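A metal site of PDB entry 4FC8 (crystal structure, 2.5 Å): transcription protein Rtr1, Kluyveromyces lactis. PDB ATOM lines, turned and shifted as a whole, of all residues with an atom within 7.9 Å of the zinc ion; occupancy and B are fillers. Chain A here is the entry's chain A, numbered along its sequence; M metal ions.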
ATOM      1  N   ARG A  67     -19.612   4.190  25.379  1.00  0.00           N
ATOM      2  CA  ARG A  67     -18.344   3.968  24.647  1.00  0.00           C
ATOM      3  C   ARG A  67     -18.157   4.921  23.462  1.00  0.00           C
ATOM      4  O   ARG A  67     -17.053   5.430  23.251  1.00  0.00           O
ATOM      5  CB  ARG A  67     -18.180   2.506  24.215  1.00  0.00           C
ATOM      6  CG  ARG A  67     -17.668   1.588  25.332  1.00  0.00           C
ATOM      7  CD  ARG A  67     -17.620   0.089  24.977  1.00  0.00           C
ATOM      8  NE  ARG A  67     -16.642  -0.227  23.935  1.00  0.00           N
ATOM      9  CZ  ARG A  67     -15.326  -0.347  24.124  1.00  0.00           C
ATOM     10  NH1 ARG A  67     -14.801  -0.194  25.319  1.00  0.00           N
ATOM     11  NH2 ARG A  67     -14.537  -0.618  23.100  1.00  0.00           N
ATOM     12  N   ARG A  72     -14.871   5.352  21.508  1.00  0.00           N
ATOM     13  CA  ARG A  72     -14.569   3.968  21.170  1.00  0.00           C
ATOM     14  C   ARG A  72     -15.742   3.210  20.534  1.00  0.00           C
ATOM     15  O   ARG A  72     -16.922   3.468  20.843  1.00  0.00           O
ATOM     16  CB  ARG A  72     -13.926   3.200  22.340  1.00  0.00           C
ATOM     17  CG  ARG A  72     -12.376   3.237  22.272  1.00  0.00           C
ATOM     18  CD  ARG A  72     -11.753   2.178  23.151  1.00  0.00           C
ATOM     19  NE  ARG A  72     -11.971   2.472  24.569  1.00  0.00           N
ATOM     20  CZ  ARG A  72     -10.998   2.698  25.457  1.00  0.00           C
ATOM     21  NH1 ARG A  72      -9.723   2.640  25.096  1.00  0.00           N
ATOM     22  NH2 ARG A  72     -11.308   2.969  26.723  1.00  0.00           N
ATOM     23  N   CYS A  73     -15.380   2.328  19.616  1.00  0.00           N
ATOM     24  CA  CYS A  73     -16.304   1.411  18.985  1.00  0.00           C
ATOM     25  C   CYS A  73     -17.128   0.782  20.106  1.00  0.00           C
ATOM     26  O   CYS A  73     -16.627   0.524  21.206  1.00  0.00           O
ATOM     27  CB  CYS A  73     -15.548   0.335  18.210  1.00  0.00           C
ATOM     28  SG  CYS A  73     -16.580  -0.815  17.211  1.00  0.00           S
ATOM     29  N   GLY A  74     -18.409   0.588  19.807  1.00  0.00           N
ATOM     30  CA  GLY A  74     -19.353   0.071  20.788  1.00  0.00           C
ATOM     31  C   GLY A  74     -19.080  -1.360  21.198  1.00  0.00           C
ATOM     32  O   GLY A  74     -19.360  -1.708  22.333  1.00  0.00           O
ATOM     33  N   TYR A  75     -18.559  -2.176  20.290  1.00  0.00           N
ATOM     34  CA  TYR A  75     -18.192  -3.565  20.603  1.00  0.00           C
ATOM     35  C   TYR A  75     -17.037  -3.616  21.603  1.00  0.00           C
ATOM     36  O   TYR A  75     -15.943  -3.149  21.286  1.00  0.00           O
ATOM     37  CB  TYR A  75     -17.787  -4.282  19.333  1.00  0.00           C
ATOM     38  CG  TYR A  75     -17.792  -5.814  19.409  1.00  0.00           C
ATOM     39  CD1 TYR A  75     -18.880  -6.541  19.934  1.00  0.00           C
ATOM     40  CD2 TYR A  75     -16.743  -6.537  18.845  1.00  0.00           C
ATOM     41  CE1 TYR A  75     -18.870  -7.914  19.938  1.00  0.00           C
ATOM     42  CE2 TYR A  75     -16.758  -7.919  18.815  1.00  0.00           C
ATOM     43  CZ  TYR A  75     -17.792  -8.613  19.374  1.00  0.00           C
ATOM     44  OH  TYR A  75     -17.731 -10.018  19.331  1.00  0.00           O
ATOM     45  N   PRO A  76     -17.249  -4.201  22.815  1.00  0.00           N
ATOM     46  CA  PRO A  76     -16.317  -3.945  23.894  1.00  0.00           C
ATOM     47  C   PRO A  76     -14.920  -4.477  23.689  1.00  0.00           C
ATOM     48  O   PRO A  76     -14.004  -4.044  24.392  1.00  0.00           O
ATOM     49  CB  PRO A  76     -16.996  -4.618  25.083  1.00  0.00           C
ATOM     50  CG  PRO A  76     -18.444  -4.387  24.790  1.00  0.00           C
ATOM     51  CD  PRO A  76     -18.488  -4.799  23.344  1.00  0.00           C
ATOM     52  N   LEU A  77     -14.762  -5.396  22.732  1.00  0.00           N
ATOM     53  CA  LEU A  77     -13.505  -6.048  22.436  1.00  0.00           C
ATOM     54  C   LEU A  77     -12.591  -5.170  21.603  1.00  0.00           C
ATOM     55  O   LEU A  77     -11.427  -5.513  21.416  1.00  0.00           O
ATOM     56  CB  LEU A  77     -13.747  -7.293  21.597  1.00  0.00           C
ATOM     57  CG  LEU A  77     -13.906  -8.647  22.253  1.00  0.00           C
ATOM     58  CD1 LEU A  77     -14.274  -9.715  21.180  1.00  0.00           C
ATOM     59  CD2 LEU A  77     -12.667  -9.049  23.055  1.00  0.00           C
ATOM     60  N   CYS A  78     -13.119  -4.045  21.093  1.00  0.00           N
ATOM     61  CA  CYS A  78     -12.443  -3.230  20.065  1.00  0.00           C
ATOM     62  C   CYS A  78     -11.649  -2.070  20.635  1.00  0.00           C
ATOM     63  O   CYS A  78     -12.207  -1.175  21.308  1.00  0.00           O
ATOM     64  CB  CYS A  78     -13.470  -2.690  19.082  1.00  0.00           C
ATOM     65  SG  CYS A  78     -12.820  -1.949  17.575  1.00  0.00           S
ATOM     66  N   SER A  79     -10.351  -2.085  20.362  1.00  0.00           N
ATOM     67  CA  SER A  79      -9.458  -1.028  20.809  1.00  0.00           C
ATOM     68  C   SER A  79      -9.572   0.195  19.903  1.00  0.00           C
ATOM     69  O   SER A  79      -9.089   1.279  20.271  1.00  0.00           O
ATOM     70  CB  SER A  79      -8.012  -1.547  20.867  1.00  0.00           C
ATOM     71  OG  SER A  79      -7.699  -2.318  19.723  1.00  0.00           O
ATOM     72  N   LYS A  80     -10.189   0.041  18.720  1.00  0.00           N
ATOM     73  CA  LYS A  80     -10.400   1.175  17.809  1.00  0.00           C
ATOM     74  C   LYS A  80     -11.630   1.975  18.189  1.00  0.00           C
ATOM     75  O   LYS A  80     -12.446   1.563  19.041  1.00  0.00           O
ATOM     76  CB  LYS A  80     -10.531   0.760  16.346  1.00  0.00           C
ATOM     77  CG  LYS A  80      -9.229   0.340  15.679  1.00  0.00           C
ATOM     78  CD  LYS A  80      -9.241  -1.181  15.390  1.00  0.00           C
ATOM     79  CE  LYS A  80     -10.043  -1.541  14.120  1.00  0.00           C
ATOM     80  NZ  LYS A  80      -9.268  -1.196  12.878  1.00  0.00           N
ATOM     81  N   SER A  81     -11.748   3.128  17.546  1.00  0.00           N
ATOM     82  CA  SER A  81     -12.870   4.022  17.732  1.00  0.00           C
ATOM     83  C   SER A  81     -13.910   3.683  16.673  1.00  0.00           C
ATOM     84  O   SER A  81     -13.657   2.853  15.785  1.00  0.00           O
ATOM     85  CB  SER A  81     -12.425   5.476  17.601  1.00  0.00           C
ATOM     86  OG  SER A  81     -11.645   5.624  16.426  1.00  0.00           O
ATOM     87  N   GLN A  82     -15.059   4.328  16.804  1.00  0.00           N
ATOM     88  CA  GLN A  82     -16.150   4.321  15.835  1.00  0.00           C
ATOM     89  C   GLN A  82     -15.683   4.856  14.461  1.00  0.00           C
ATOM     90  O   GLN A  82     -14.558   5.350  14.346  1.00  0.00           O
ATOM     91  CB  GLN A  82     -17.286   5.183  16.398  1.00  0.00           C
ATOM     92  CG  GLN A  82     -16.736   6.437  17.075  1.00  0.00           C
ATOM     93  CD  GLN A  82     -17.686   7.079  18.043  1.00  0.00           C
ATOM     94  OE1 GLN A  82     -17.383   7.181  19.235  1.00  0.00           O
ATOM     95  NE2 GLN A  82     -18.857   7.508  17.552  1.00  0.00           N
ATOM     96  N   ALA A  83     -16.535   4.732  13.432  1.00  0.00           N
ATOM     97  CA  ALA A  83     -16.208   5.230  12.089  1.00  0.00           C
ATOM     98  C   ALA A  83     -16.392   6.750  11.958  1.00  0.00           C
ATOM     99  O   ALA A  83     -15.493   7.470  11.480  1.00  0.00           O
ATOM    100  CB  ALA A  83     -17.017   4.476  11.019  1.00  0.00           C
ATOM    101  N   GLU A 109     -21.855   4.220  15.823  1.00  0.00           N
ATOM    102  CA  GLU A 109     -21.722   3.324  16.976  1.00  0.00           C
ATOM    103  C   GLU A 109     -20.526   2.381  16.874  1.00  0.00           C
ATOM    104  O   GLU A 109     -19.971   1.999  17.897  1.00  0.00           O
ATOM    105  CB  GLU A 109     -23.032   2.577  17.221  1.00  0.00           C
ATOM    106  CG  GLU A 109     -24.143   3.509  17.694  1.00  0.00           C
ATOM    107  CD  GLU A 109     -25.548   2.964  17.525  1.00  0.00           C
ATOM    108  OE1 GLU A 109     -25.732   1.835  17.014  1.00  0.00           O
ATOM    109  OE2 GLU A 109     -26.474   3.721  17.919  1.00  0.00           O
ATOM    110  N   TYR A 110     -20.131   2.046  15.643  1.00  0.00           N
ATOM    111  CA  TYR A 110     -19.120   1.005  15.397  1.00  0.00           C
ATOM    112  C   TYR A 110     -18.075   1.417  14.389  1.00  0.00           C
ATOM    113  O   TYR A 110     -18.298   2.337  13.616  1.00  0.00           O
ATOM    114  CB  TYR A 110     -19.809  -0.257  14.939  1.00  0.00           C
ATOM    115  CG  TYR A 110     -20.777  -0.743  15.965  1.00  0.00           C
ATOM    116  CD1 TYR A 110     -20.332  -1.436  17.114  1.00  0.00           C
ATOM    117  CD2 TYR A 110     -22.141  -0.493  15.830  1.00  0.00           C
ATOM    118  CE1 TYR A 110     -21.231  -1.872  18.087  1.00  0.00           C
ATOM    119  CE2 TYR A 110     -23.062  -0.925  16.798  1.00  0.00           C
ATOM    120  CZ  TYR A 110     -22.590  -1.625  17.922  1.00  0.00           C
ATOM    121  OH  TYR A 110     -23.485  -2.047  18.860  1.00  0.00           O
ATOM    122  N   CYS A 111     -16.938   0.727  14.395  1.00  0.00           N
ATOM    123  CA  CYS A 111     -15.830   1.046  13.509  1.00  0.00           C
ATOM    124  C   CYS A 111     -16.143   0.612  12.093  1.00  0.00           C
ATOM    125  O   CYS A 111     -15.829   1.304  11.119  1.00  0.00           O
ATOM    126  CB  CYS A 111     -14.536   0.356  13.974  1.00  0.00           C
ATOM    127  SG  CYS A 111     -14.685  -1.469  13.999  1.00  0.00           S
ATOM    128  N   THR A 112     -16.773  -0.552  11.968  1.00  0.00           N
ATOM    129  CA  THR A 112     -16.990  -1.192  10.699  1.00  0.00           C
ATOM    130  C   THR A 112     -18.397  -1.772  10.701  1.00  0.00           C
ATOM    131  O   THR A 112     -19.055  -1.786  11.742  1.00  0.00           O
ATOM    132  CB  THR A 112     -15.979  -2.326  10.504  1.00  0.00           C
ATOM    133  OG1 THR A 112     -15.979  -3.172  11.659  1.00  0.00           O
ATOM    134  CG2 THR A 112     -14.560  -1.774  10.296  1.00  0.00           C
ATOM    135  N   ALA A 114     -18.748  -4.886  10.335  1.00  0.00           N
ATOM    136  CA  ALA A 114     -18.507  -6.208  10.916  1.00  0.00           C
ATOM    137  C   ALA A 114     -18.636  -6.190  12.425  1.00  0.00           C
ATOM    138  O   ALA A 114     -19.182  -7.121  13.006  1.00  0.00           O
ATOM    139  CB  ALA A 114     -17.142  -6.749  10.486  1.00  0.00           C
ATOM    140  N   HIS A 115     -18.133  -5.132  13.063  1.00  0.00           N
ATOM    141  CA  HIS A 115     -18.315  -5.037  14.499  1.00  0.00           C
ATOM    142  C   HIS A 115     -19.756  -4.707  14.880  1.00  0.00           C
ATOM    143  O   HIS A 115     -20.191  -5.098  15.959  1.00  0.00           O
ATOM    144  CB  HIS A 115     -17.284  -4.123  15.151  1.00  0.00           C
ATOM    145  CG  HIS A 115     -15.970  -4.804  15.412  1.00  0.00           C
ATOM    146  ND1 HIS A 115     -14.846  -4.129  15.837  1.00  0.00           N
ATOM    147  CD2 HIS A 115     -15.599  -6.102  15.278  1.00  0.00           C
ATOM    148  CE1 HIS A 115     -13.847  -4.985  15.971  1.00  0.00           C
ATOM    149  NE2 HIS A 115     -14.276  -6.189  15.630  1.00  0.00           N
ATOM    150  N   PHE A 116     -20.497  -4.066  13.976  1.00  0.00           N
ATOM    151  CA  PHE A 116     -21.921  -3.869  14.183  1.00  0.00           C
ATOM    152  C   PHE A 116     -22.657  -5.214  14.344  1.00  0.00           C
ATOM    153  O   PHE A 116     -23.398  -5.408  15.315  1.00  0.00           O
ATOM    154  CB  PHE A 116     -22.540  -3.066  13.032  1.00  0.00           C
ATOM    155  CG  PHE A 116     -24.038  -3.067  13.017  1.00  0.00           C
ATOM    156  CD1 PHE A 116     -24.758  -2.539  14.082  1.00  0.00           C
ATOM    157  CD2 PHE A 116     -24.733  -3.592  11.936  1.00  0.00           C
ATOM    158  CE1 PHE A 116     -26.156  -2.538  14.083  1.00  0.00           C
ATOM    159  CE2 PHE A 116     -26.147  -3.597  11.915  1.00  0.00           C
ATOM    160  CZ  PHE A 116     -26.850  -3.063  13.003  1.00  0.00           C
HETATM  161 ZN    ZN M   1     -14.724  -1.971  16.394  1.00  0.00          ZN
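The zinc ion is bound by a ring nitrogen (ND1) of His 115 (2.2 Å).
The zinc ion is bound by SG of Cys 78.
SG of Cys 73 binds the zinc ion, 2.3 Å away.
The zinc ion is bound by the side-chain sulfur (SG) of Cys 111.
The backbone NH (N) of His 115 sits at hydrogen-bond distance from the side-chain hydroxyl (OG1) of Thr 112, 3.2 Å away.
The side-chain sulfur of Cys 78 lies close to the backbone NH of Lys 80, 3.5 Å away.
O of Cys 78 sits at hydrogen-bond distance from NH2 of Arg 67, 3.0 Å away.
The backbone NH of Cys 73 lies within hydrogen-bond range of the backbone carbonyl oxygen of Lys 80, at 3.1 Å.
NE of Arg 67 sits at hydrogen-bond distance from O of Cys 73 (2.8 Å).
The side-chain sulfur of Cys 111 lies close to the side-chain hydroxyl of Thr 112 (3.2 Å).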
